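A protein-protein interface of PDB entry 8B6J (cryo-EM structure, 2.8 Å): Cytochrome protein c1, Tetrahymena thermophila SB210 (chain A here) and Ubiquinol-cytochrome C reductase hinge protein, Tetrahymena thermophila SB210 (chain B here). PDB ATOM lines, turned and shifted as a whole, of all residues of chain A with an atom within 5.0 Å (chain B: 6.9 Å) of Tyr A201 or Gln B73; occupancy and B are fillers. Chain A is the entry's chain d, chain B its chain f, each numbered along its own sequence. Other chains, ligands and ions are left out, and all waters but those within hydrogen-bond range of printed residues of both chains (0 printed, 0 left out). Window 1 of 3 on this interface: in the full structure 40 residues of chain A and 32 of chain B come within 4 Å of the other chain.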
ATOM      1  N   LEU A  43      18.474  15.372  22.715  1.00  0.00           N
ATOM      2  CA  LEU A  43      17.862  14.602  21.641  1.00  0.00           C
ATOM      3  C   LEU A  43      16.875  13.618  22.250  1.00  0.00           C
ATOM      4  O   LEU A  43      16.833  13.418  23.465  1.00  0.00           O
ATOM      5  CB  LEU A  43      18.923  13.882  20.803  1.00  0.00           C
ATOM      6  CG  LEU A  43      19.783  12.847  21.531  1.00  0.00           C
ATOM      7  CD1 LEU A  43      19.249  11.450  21.305  1.00  0.00           C
ATOM      8  CD2 LEU A  43      21.228  12.940  21.085  1.00  0.00           C
ATOM      9  N   VAL A  44      16.076  13.007  21.382  1.00  0.00           N
ATOM     10  CA  VAL A  44      15.060  12.045  21.793  1.00  0.00           C
ATOM     11  C   VAL A  44      15.687  10.659  21.838  1.00  0.00           C
ATOM     12  O   VAL A  44      16.259  10.193  20.845  1.00  0.00           O
ATOM     13  CB  VAL A  44      13.858  12.072  20.836  1.00  0.00           C
ATOM     14  CG1 VAL A  44      12.777  11.121  21.318  1.00  0.00           C
ATOM     15  CG2 VAL A  44      13.313  13.484  20.698  1.00  0.00           C
ATOM     16  N   VAL A  47      11.994   7.157  22.375  1.00  0.00           N
ATOM     17  CA  VAL A  47      10.851   7.218  21.465  1.00  0.00           C
ATOM     18  C   VAL A  47      10.227   5.841  21.284  1.00  0.00           C
ATOM     19  O   VAL A  47       9.007   5.676  21.400  1.00  0.00           O
ATOM     20  CB  VAL A  47      11.272   7.822  20.114  1.00  0.00           C
ATOM     21  CG1 VAL A  47      12.356   6.976  19.452  1.00  0.00           C
ATOM     22  CG2 VAL A  47      10.068   7.947  19.204  1.00  0.00           C
ATOM     23  N   ASN A  54       8.155  -0.278  19.577  1.00  0.00           N
ATOM     24  CA  ASN A  54       8.175  -0.623  18.163  1.00  0.00           C
ATOM     25  C   ASN A  54       8.563  -2.089  18.028  1.00  0.00           C
ATOM     26  O   ASN A  54       9.631  -2.499  18.494  1.00  0.00           O
ATOM     27  CB  ASN A  54       9.155   0.267  17.405  1.00  0.00           C
ATOM     28  CG  ASN A  54       8.877   1.741  17.605  1.00  0.00           C
ATOM     29  OD1 ASN A  54       7.797   2.127  18.050  1.00  0.00           O
ATOM     30  ND2 ASN A  54       9.852   2.577  17.272  1.00  0.00           N
ATOM     31  N   TYR A 174      17.176   3.680  16.398  1.00  0.00           N
ATOM     32  CA  TYR A 174      17.838   4.916  15.995  1.00  0.00           C
ATOM     33  C   TYR A 174      17.703   5.150  14.494  1.00  0.00           C
ATOM     34  O   TYR A 174      17.114   6.144  14.055  1.00  0.00           O
ATOM     35  CB  TYR A 174      19.309   4.869  16.407  1.00  0.00           C
ATOM     36  CG  TYR A 174      20.051   6.165  16.181  1.00  0.00           C
ATOM     37  CD1 TYR A 174      19.908   7.227  17.060  1.00  0.00           C
ATOM     38  CD2 TYR A 174      20.899   6.324  15.096  1.00  0.00           C
ATOM     39  CE1 TYR A 174      20.583   8.410  16.863  1.00  0.00           C
ATOM     40  CE2 TYR A 174      21.579   7.504  14.892  1.00  0.00           C
ATOM     41  CZ  TYR A 174      21.418   8.543  15.779  1.00  0.00           C
ATOM     42  OH  TYR A 174      22.091   9.724  15.581  1.00  0.00           O
ATOM     43  N   TYR A 176      15.783   3.937  12.367  1.00  0.00           N
ATOM     44  CA  TYR A 176      14.396   4.113  11.956  1.00  0.00           C
ATOM     45  C   TYR A 176      13.894   5.511  12.287  1.00  0.00           C
ATOM     46  O   TYR A 176      13.187   6.127  11.482  1.00  0.00           O
ATOM     47  CB  TYR A 176      13.514   3.058  12.620  1.00  0.00           C
ATOM     48  CG  TYR A 176      12.059   3.169  12.232  1.00  0.00           C
ATOM     49  CD1 TYR A 176      11.634   2.817  10.959  1.00  0.00           C
ATOM     50  CD2 TYR A 176      11.114   3.624  13.137  1.00  0.00           C
ATOM     51  CE1 TYR A 176      10.307   2.919  10.599  1.00  0.00           C
ATOM     52  CE2 TYR A 176       9.785   3.727  12.786  1.00  0.00           C
ATOM     53  CZ  TYR A 176       9.386   3.374  11.516  1.00  0.00           C
ATOM     54  OH  TYR A 176       8.062   3.476  11.163  1.00  0.00           O
ATOM     55  N   ASN A 177      14.240   6.030  13.465  1.00  0.00           N
ATOM     56  CA  ASN A 177      13.697   7.321  13.875  1.00  0.00           C
ATOM     57  C   ASN A 177      14.247   8.450  13.013  1.00  0.00           C
ATOM     58  O   ASN A 177      13.482   9.249  12.459  1.00  0.00           O
ATOM     59  CB  ASN A 177      13.999   7.569  15.352  1.00  0.00           C
ATOM     60  CG  ASN A 177      13.300   6.582  16.261  1.00  0.00           C
ATOM     61  OD1 ASN A 177      13.934   5.919  17.081  1.00  0.00           O
ATOM     62  ND2 ASN A 177      11.985   6.479  16.123  1.00  0.00           N
ATOM     63  N   ILE A 178      15.571   8.522  12.866  1.00  0.00           N
ATOM     64  CA  ILE A 178      16.165   9.605  12.088  1.00  0.00           C
ATOM     65  C   ILE A 178      15.689   9.542  10.644  1.00  0.00           C
ATOM     66  O   ILE A 178      15.389  10.572  10.028  1.00  0.00           O
ATOM     67  CB  ILE A 178      17.701   9.561  12.187  1.00  0.00           C
ATOM     68  CG1 ILE A 178      18.147  10.193  13.508  1.00  0.00           C
ATOM     69  CG2 ILE A 178      18.339  10.265  10.987  1.00  0.00           C
ATOM     70  CD1 ILE A 178      19.641  10.267  13.697  1.00  0.00           C
ATOM     71  N   THR A 180      12.937   8.766   9.635  1.00  0.00           N
ATOM     72  CA  THR A 180      11.535   9.155   9.576  1.00  0.00           C
ATOM     73  C   THR A 180      11.240  10.501  10.217  1.00  0.00           C
ATOM     74  O   THR A 180      10.376  11.226   9.722  1.00  0.00           O
ATOM     75  CB  THR A 180      10.669   8.086  10.257  1.00  0.00           C
ATOM     76  OG1 THR A 180      10.950   6.804   9.684  1.00  0.00           O
ATOM     77  CG2 THR A 180       9.196   8.394  10.080  1.00  0.00           C
ATOM     78  N   GLY A 181      11.938  10.857  11.291  1.00  0.00           N
ATOM     79  CA  GLY A 181      11.612  12.051  12.044  1.00  0.00           C
ATOM     80  C   GLY A 181      12.142  13.337  11.448  1.00  0.00           C
ATOM     81  O   GLY A 181      13.082  13.931  11.982  1.00  0.00           O
ATOM     82  N   ASN A 199      16.111  17.631  12.854  1.00  0.00           N
ATOM     83  CA  ASN A 199      15.679  16.267  13.124  1.00  0.00           C
ATOM     84  C   ASN A 199      15.785  16.014  14.623  1.00  0.00           C
ATOM     85  O   ASN A 199      16.898  15.909  15.151  1.00  0.00           O
ATOM     86  CB  ASN A 199      16.528  15.264  12.342  1.00  0.00           C
ATOM     87  CG  ASN A 199      15.988  13.854  12.426  1.00  0.00           C
ATOM     88  OD1 ASN A 199      15.377  13.467  13.419  1.00  0.00           O
ATOM     89  ND2 ASN A 199      16.210  13.074  11.377  1.00  0.00           N
ATOM     90  N   PRO A 200      14.667  15.895  15.343  1.00  0.00           N
ATOM     91  CA  PRO A 200      14.746  15.880  16.814  1.00  0.00           C
ATOM     92  C   PRO A 200      15.536  14.715  17.387  1.00  0.00           C
ATOM     93  O   PRO A 200      15.956  14.792  18.547  1.00  0.00           O
ATOM     94  CB  PRO A 200      13.274  15.823  17.243  1.00  0.00           C
ATOM     95  CG  PRO A 200      12.559  15.250  16.080  1.00  0.00           C
ATOM     96  CD  PRO A 200      13.282  15.743  14.869  1.00  0.00           C
ATOM     97  N   TYR A 201      15.750  13.643  16.628  1.00  0.00           N
ATOM     98  CA  TYR A 201      16.438  12.474  17.162  1.00  0.00           C
ATOM     99  C   TYR A 201      17.955  12.584  17.106  1.00  0.00           C
ATOM    100  O   TYR A 201      18.637  11.758  17.722  1.00  0.00           O
ATOM    101  CB  TYR A 201      16.005  11.222  16.404  1.00  0.00           C
ATOM    102  CG  TYR A 201      14.529  10.936  16.494  1.00  0.00           C
ATOM    103  CD1 TYR A 201      13.988  10.334  17.619  1.00  0.00           C
ATOM    104  CD2 TYR A 201      13.677  11.258  15.450  1.00  0.00           C
ATOM    105  CE1 TYR A 201      12.641  10.069  17.705  1.00  0.00           C
ATOM    106  CE2 TYR A 201      12.329  10.995  15.527  1.00  0.00           C
ATOM    107  CZ  TYR A 201      11.817  10.400  16.656  1.00  0.00           C
ATOM    108  OH  TYR A 201      10.473  10.138  16.729  1.00  0.00           O
ATOM    109  N   PHE A 202      18.499  13.564  16.395  1.00  0.00           N
ATOM    110  CA  PHE A 202      19.938  13.682  16.233  1.00  0.00           C
ATOM    111  C   PHE A 202      20.531  14.558  17.332  1.00  0.00           C
ATOM    112  O   PHE A 202      19.843  15.369  17.955  1.00  0.00           O
ATOM    113  CB  PHE A 202      20.274  14.259  14.858  1.00  0.00           C
ATOM    114  CG  PHE A 202      21.734  14.195  14.518  1.00  0.00           C
ATOM    115  CD1 PHE A 202      22.296  13.023  14.050  1.00  0.00           C
ATOM    116  CD2 PHE A 202      22.542  15.308  14.663  1.00  0.00           C
ATOM    117  CE1 PHE A 202      23.637  12.961  13.736  1.00  0.00           C
ATOM    118  CE2 PHE A 202      23.883  15.251  14.350  1.00  0.00           C
ATOM    119  CZ  PHE A 202      24.431  14.076  13.886  1.00  0.00           C
ATOM    120  N   ASP A 203      21.828  14.375  17.569  1.00  0.00           N
ATOM    121  CA  ASP A 203      22.532  15.164  18.572  1.00  0.00           C
ATOM    122  C   ASP A 203      22.313  16.647  18.325  1.00  0.00           C
ATOM    123  O   ASP A 203      22.683  17.173  17.272  1.00  0.00           O
ATOM    124  CB  ASP A 203      24.027  14.837  18.542  1.00  0.00           C
ATOM    125  CG  ASP A 203      24.304  13.359  18.723  1.00  0.00           C
ATOM    126  OD1 ASP A 203      23.337  12.584  18.880  1.00  0.00           O
ATOM    127  OD2 ASP A 203      25.490  12.968  18.705  1.00  0.00           O
ATOM    128  N   LYS B  20       2.553   9.097   8.362  1.00  0.00           N
ATOM    129  CA  LYS B  20       3.071   9.775   9.547  1.00  0.00           C
ATOM    130  C   LYS B  20       2.350  11.092   9.804  1.00  0.00           C
ATOM    131  O   LYS B  20       2.114  11.453  10.961  1.00  0.00           O
ATOM    132  CB  LYS B  20       4.574  10.008   9.418  1.00  0.00           C
ATOM    133  CG  LYS B  20       5.144  10.814  10.575  1.00  0.00           C
ATOM    134  CD  LYS B  20       6.485  10.286  11.038  1.00  0.00           C
ATOM    135  CE  LYS B  20       6.961  11.028  12.276  1.00  0.00           C
ATOM    136  NZ  LYS B  20       8.247  10.492  12.796  1.00  0.00           N
ATOM    137  N   LEU B  23      -1.201  10.318  11.195  1.00  0.00           N
ATOM    138  CA  LEU B  23      -1.113   9.791  12.551  1.00  0.00           C
ATOM    139  C   LEU B  23      -0.635  10.855  13.532  1.00  0.00           C
ATOM    140  O   LEU B  23      -1.055  10.855  14.692  1.00  0.00           O
ATOM    141  CB  LEU B  23      -0.190   8.573  12.578  1.00  0.00           C
ATOM    142  CG  LEU B  23      -0.612   7.430  13.505  1.00  0.00           C
ATOM    143  CD1 LEU B  23      -2.018   6.950  13.185  1.00  0.00           C
ATOM    144  CD2 LEU B  23       0.370   6.281  13.399  1.00  0.00           C
ATOM    145  N   CYS B  27      -2.724  11.886  16.789  1.00  0.00           N
ATOM    146  CA  CYS B  27      -2.136  11.734  18.114  1.00  0.00           C
ATOM    147  C   CYS B  27      -1.821  13.057  18.798  1.00  0.00           C
ATOM    148  O   CYS B  27      -1.475  13.052  19.984  1.00  0.00           O
ATOM    149  CB  CYS B  27      -0.849  10.904  18.025  1.00  0.00           C
ATOM    150  SG  CYS B  27      -1.077   9.244  17.349  1.00  0.00           S
ATOM    151  N   VAL B  65       7.879  16.064  21.488  1.00  0.00           N
ATOM    152  CA  VAL B  65       8.075  15.160  20.362  1.00  0.00           C
ATOM    153  C   VAL B  65       8.201  13.726  20.850  1.00  0.00           C
ATOM    154  O   VAL B  65       7.723  12.795  20.196  1.00  0.00           O
ATOM    155  CB  VAL B  65       9.297  15.584  19.526  1.00  0.00           C
ATOM    156  CG1 VAL B  65       9.112  16.991  18.983  1.00  0.00           C
ATOM    157  CG2 VAL B  65      10.573  15.481  20.343  1.00  0.00           C
ATOM    158  N   THR B  66       8.839  13.518  22.004  1.00  0.00           N
ATOM    159  CA  THR B  66       8.931  12.172  22.555  1.00  0.00           C
ATOM    160  C   THR B  66       7.546  11.612  22.838  1.00  0.00           C
ATOM    161  O   THR B  66       7.240  10.470  22.481  1.00  0.00           O
ATOM    162  CB  THR B  66       9.770  12.185  23.834  1.00  0.00           C
ATOM    163  OG1 THR B  66      11.050  12.770  23.567  1.00  0.00           O
ATOM    164  CG2 THR B  66       9.965  10.771  24.359  1.00  0.00           C
ATOM    165  N   ILE B  68       4.631  12.513  21.534  1.00  0.00           N
ATOM    166  CA  ILE B  68       3.872  12.289  20.304  1.00  0.00           C
ATOM    167  C   ILE B  68       4.375  11.043  19.583  1.00  0.00           C
ATOM    168  O   ILE B  68       3.589  10.190  19.146  1.00  0.00           O
ATOM    169  CB  ILE B  68       3.946  13.528  19.393  1.00  0.00           C
ATOM    170  CG1 ILE B  68       3.117  14.678  19.971  1.00  0.00           C
ATOM    171  CG2 ILE B  68       3.478  13.187  17.989  1.00  0.00           C
ATOM    172  CD1 ILE B  68       1.623  14.407  20.039  1.00  0.00           C
ATOM    173  N   GLU B  69       5.694  10.916  19.447  1.00  0.00           N
ATOM    174  CA  GLU B  69       6.253   9.815  18.680  1.00  0.00           C
ATOM    175  C   GLU B  69       6.083   8.485  19.397  1.00  0.00           C
ATOM    176  O   GLU B  69       5.923   7.453  18.740  1.00  0.00           O
ATOM    177  CB  GLU B  69       7.725  10.092  18.389  1.00  0.00           C
ATOM    178  CG  GLU B  69       7.936  11.285  17.475  1.00  0.00           C
ATOM    179  CD  GLU B  69       7.690  10.946  16.019  1.00  0.00           C
ATOM    180  OE1 GLU B  69       8.292   9.970  15.527  1.00  0.00           O
ATOM    181  OE2 GLU B  69       6.890  11.647  15.368  1.00  0.00           O
ATOM    182  N   ALA B  70       6.080   8.484  20.732  1.00  0.00           N
ATOM    183  CA  ALA B  70       5.882   7.242  21.464  1.00  0.00           C
ATOM    184  C   ALA B  70       4.552   6.589  21.125  1.00  0.00           C
ATOM    185  O   ALA B  70       4.397   5.381  21.327  1.00  0.00           O
ATOM    186  CB  ALA B  70       5.968   7.503  22.967  1.00  0.00           C
ATOM    187  N   CYS B  71       3.592   7.359  20.618  1.00  0.00           N
ATOM    188  CA  CYS B  71       2.330   6.812  20.143  1.00  0.00           C
ATOM    189  C   CYS B  71       2.275   6.678  18.629  1.00  0.00           C
ATOM    190  O   CYS B  71       1.643   5.745  18.126  1.00  0.00           O
ATOM    191  CB  CYS B  71       1.165   7.691  20.609  1.00  0.00           C
ATOM    192  SG  CYS B  71       1.027   7.850  22.404  1.00  0.00           S
ATOM    193  N   VAL B  72       2.916   7.586  17.892  1.00  0.00           N
ATOM    194  CA  VAL B  72       2.870   7.512  16.434  1.00  0.00           C
ATOM    195  C   VAL B  72       3.665   6.311  15.926  1.00  0.00           C
ATOM    196  O   VAL B  72       3.167   5.514  15.123  1.00  0.00           O
ATOM    197  CB  VAL B  72       3.380   8.825  15.814  1.00  0.00           C
ATOM    198  CG1 VAL B  72       3.517   8.686  14.306  1.00  0.00           C
ATOM    199  CG2 VAL B  72       2.443   9.968  16.155  1.00  0.00           C
ATOM    200  N   GLN B  73       4.910   6.163  16.383  1.00  0.00           N
ATOM    201  CA  GLN B  73       5.811   5.180  15.784  1.00  0.00           C
ATOM    202  C   GLN B  73       5.335   3.745  15.951  1.00  0.00           C
ATOM    203  O   GLN B  73       5.298   3.010  14.948  1.00  0.00           O
ATOM    204  CB  GLN B  73       7.219   5.357  16.364  1.00  0.00           C
ATOM    205  CG  GLN B  73       7.881   6.680  16.021  1.00  0.00           C
ATOM    206  CD  GLN B  73       8.302   6.767  14.569  1.00  0.00           C
ATOM    207  OE1 GLN B  73       7.916   5.938  13.748  1.00  0.00           O
ATOM    208  NE2 GLN B  73       9.103   7.775  14.246  1.00  0.00           N
ATOM    209  N   PRO B  74       4.980   3.271  17.151  1.00  0.00           N
ATOM    210  CA  PRO B  74       4.625   1.848  17.284  1.00  0.00           C
ATOM    211  C   PRO B  74       3.484   1.426  16.378  1.00  0.00           C
ATOM    212  O   PRO B  74       3.515   0.324  15.818  1.00  0.00           O
ATOM    213  CB  PRO B  74       4.252   1.720  18.768  1.00  0.00           C
ATOM    214  CG  PRO B  74       4.923   2.863  19.435  1.00  0.00           C
ATOM    215  CD  PRO B  74       4.899   3.976  18.441  1.00  0.00           C
ATOM    216  N   ALA B  75       2.473   2.282  16.214  1.00  0.00           N
ATOM    217  CA  ALA B  75       1.338   1.926  15.370  1.00  0.00           C
ATOM    218  C   ALA B  75       1.774   1.712  13.929  1.00  0.00           C
ATOM    219  O   ALA B  75       1.359   0.742  13.285  1.00  0.00           O
ATOM    220  CB  ALA B  75       0.265   3.010  15.452  1.00  0.00           C
ATOM    221  N   ILE B  76       2.613   2.605  13.405  1.00  0.00           N
ATOM    222  CA  ILE B  76       3.092   2.445  12.038  1.00  0.00           C
ATOM    223  C   ILE B  76       3.956   1.197  11.920  1.00  0.00           C
ATOM    224  O   ILE B  76       3.808   0.413  10.976  1.00  0.00           O
ATOM    225  CB  ILE B  76       3.851   3.705  11.586  1.00  0.00           C
ATOM    226  CG1 ILE B  76       2.948   4.936  11.701  1.00  0.00           C
ATOM    227  CG2 ILE B  76       4.348   3.538  10.154  1.00  0.00           C
ATOM    228  CD1 ILE B  76       3.629   6.240  11.348  1.00  0.00           C
ATOM    229  N   THR B  77       4.865   0.986  12.874  1.00  0.00           N
ATOM    230  CA  THR B  77       5.783  -0.145  12.771  1.00  0.00           C
ATOM    231  C   THR B  77       5.035  -1.474  12.807  1.00  0.00           C
ATOM    232  O   THR B  77       5.370  -2.401  12.060  1.00  0.00           O
ATOM    233  CB  THR B  77       6.824  -0.096  13.889  1.00  0.00           C
ATOM    234  OG1 THR B  77       6.165  -0.058  15.160  1.00  0.00           O
ATOM    235  CG2 THR B  77       7.715   1.127  13.737  1.00  0.00           C
ATOM    236  N   ARG B  78       4.022  -1.590  13.668  1.00  0.00           N
ATOM    237  CA  ARG B  78       3.319  -2.860  13.809  1.00  0.00           C
ATOM    238  C   ARG B  78       2.595  -3.279  12.536  1.00  0.00           C
ATOM    239  O   ARG B  78       2.257  -4.458  12.393  1.00  0.00           O
ATOM    240  CB  ARG B  78       2.323  -2.783  14.967  1.00  0.00           C
ATOM    241  CG  ARG B  78       2.949  -3.033  16.329  1.00  0.00           C
ATOM    242  CD  ARG B  78       1.901  -3.126  17.428  1.00  0.00           C
ATOM    243  NE  ARG B  78       1.439  -1.815  17.871  1.00  0.00           N
ATOM    244  CZ  ARG B  78       0.419  -1.153  17.340  1.00  0.00           C
ATOM    245  NH1 ARG B  78      -0.272  -1.641  16.324  1.00  0.00           N
ATOM    246  NH2 ARG B  78       0.084   0.032  17.844  1.00  0.00           N
ATOM    247  N   LEU B  80       3.804  -2.777   9.326  1.00  0.00           N
ATOM    248  CA  LEU B  80       4.720  -2.824   8.197  1.00  0.00           C
ATOM    249  C   LEU B  80       5.008  -4.263   7.786  1.00  0.00           C
ATOM    250  O   LEU B  80       4.993  -5.180   8.609  1.00  0.00           O
ATOM    251  CB  LEU B  80       6.033  -2.115   8.537  1.00  0.00           C
ATOM    252  CG  LEU B  80       5.944  -0.599   8.714  1.00  0.00           C
ATOM    253  CD1 LEU B  80       7.255  -0.038   9.224  1.00  0.00           C
ATOM    254  CD2 LEU B  80       5.559   0.074   7.410  1.00  0.00           C
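The backbone carbonyl oxygen of Gln B73 lies within hydrogen-bond range of the side-chain hydroxyl of Thr B77. O of Pro A200 sits at hydrogen-bond distance from N of Val A44 (3.4 Å). OG1 of Thr A180 sits at hydrogen-bond distance from O of Tyr A176, 2.9 Å away. The side-chain carboxylate (OE1) of Glu B69 is in hydrogen-bond range of the side-chain amide nitrogen (NE2) of Gln B73 (2.7 Å). O of Gly A181 lies close to OD1 of Asn A199 (2.7 Å). The side-chain amide oxygen of Asn A199 lies close to the backbone NH of Tyr A201, at 3.2 Å.
Printed residues of chain B within 4 Å of Asn A54: Gln B73 (3.6 Å), Pro B74 (3.2 Å) and Thr B77 (3.7 Å). Of the printed residues of chain B, Thr A180 touches Lys B20 (3.4 Å). Tyr A201 touches just these residues of chain B: Glu B69 (2.5 Å) and Gln B73 (3.7 Å). Leu B23 touches none of the printed residues of chain A. Printed residues of chain A within 4 Å of Thr B66: Val A44 (3.3 Å). Of chain A, only Asn A54 (3.6 Å), Tyr A176 (3.1 Å), Asn A177 (3.7 Å) and Tyr A201 (3.7 Å) come within 4 Å of Gln B73. Ala B75 touches none of the printed residues of chain A. The nearest residue of chain B that does not touch Tyr A201 is Lys B20 (4.5 Å). The nearest residue of chain A that does not touch Gln B73 is Val A47 (4.1 Å). The nearest printed residue of chain B that does not touch Val A44 is Glu B69 (5.9 Å).
The side-chain hydroxyl (OH) of Tyr A201 sits at hydrogen-bond distance from the side-chain carboxylate (OE1) of Glu B69 (2.5 Å). The side-chain amide oxygen (OD1) of Asn A54 lies close to the backbone nitrogen (N) of Pro B74 (3.2 Å).
Val B65 touches Val A44 (CG2 to CG2, 3.4 Å). Val A44 touches Thr B66 (CG1 to OG1, 3.3 Å). CG2 of Val A47 touches CB of Glu B69, at 3.3 Å. OG1 of Thr B77 touches CA of Asn A54, at 3.7 Å. Tyr A176 touches Ile B76 (OH to CG2, 3.8 Å). Tyr A176 touches Thr B77. ND2 of Asn A177 touches NE2 of Gln B73 (3.7 Å). Lys B20 touches Thr A180. Gly A181 touches Lys B20 (CA to NZ, 3.8 Å). Gln B73 touches Tyr A201 (NE2 to OH, 3.7 Å).
Of the 17 printed residues of chain B, 9 touch a printed residue of chain A. Hydrophobic or aromatic side chains of chain B within 4 Å of the printed part of chain A: Val B65, Ala B70, Pro B74 and Ile B76. Of the 15 printed residues of chain A, 8 touch a printed residue of chain B. Among the printed residues, no Asp or Glu carboxylate lies within 4 Å of a Lys or Arg side-chain nitrogen of the other chain.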
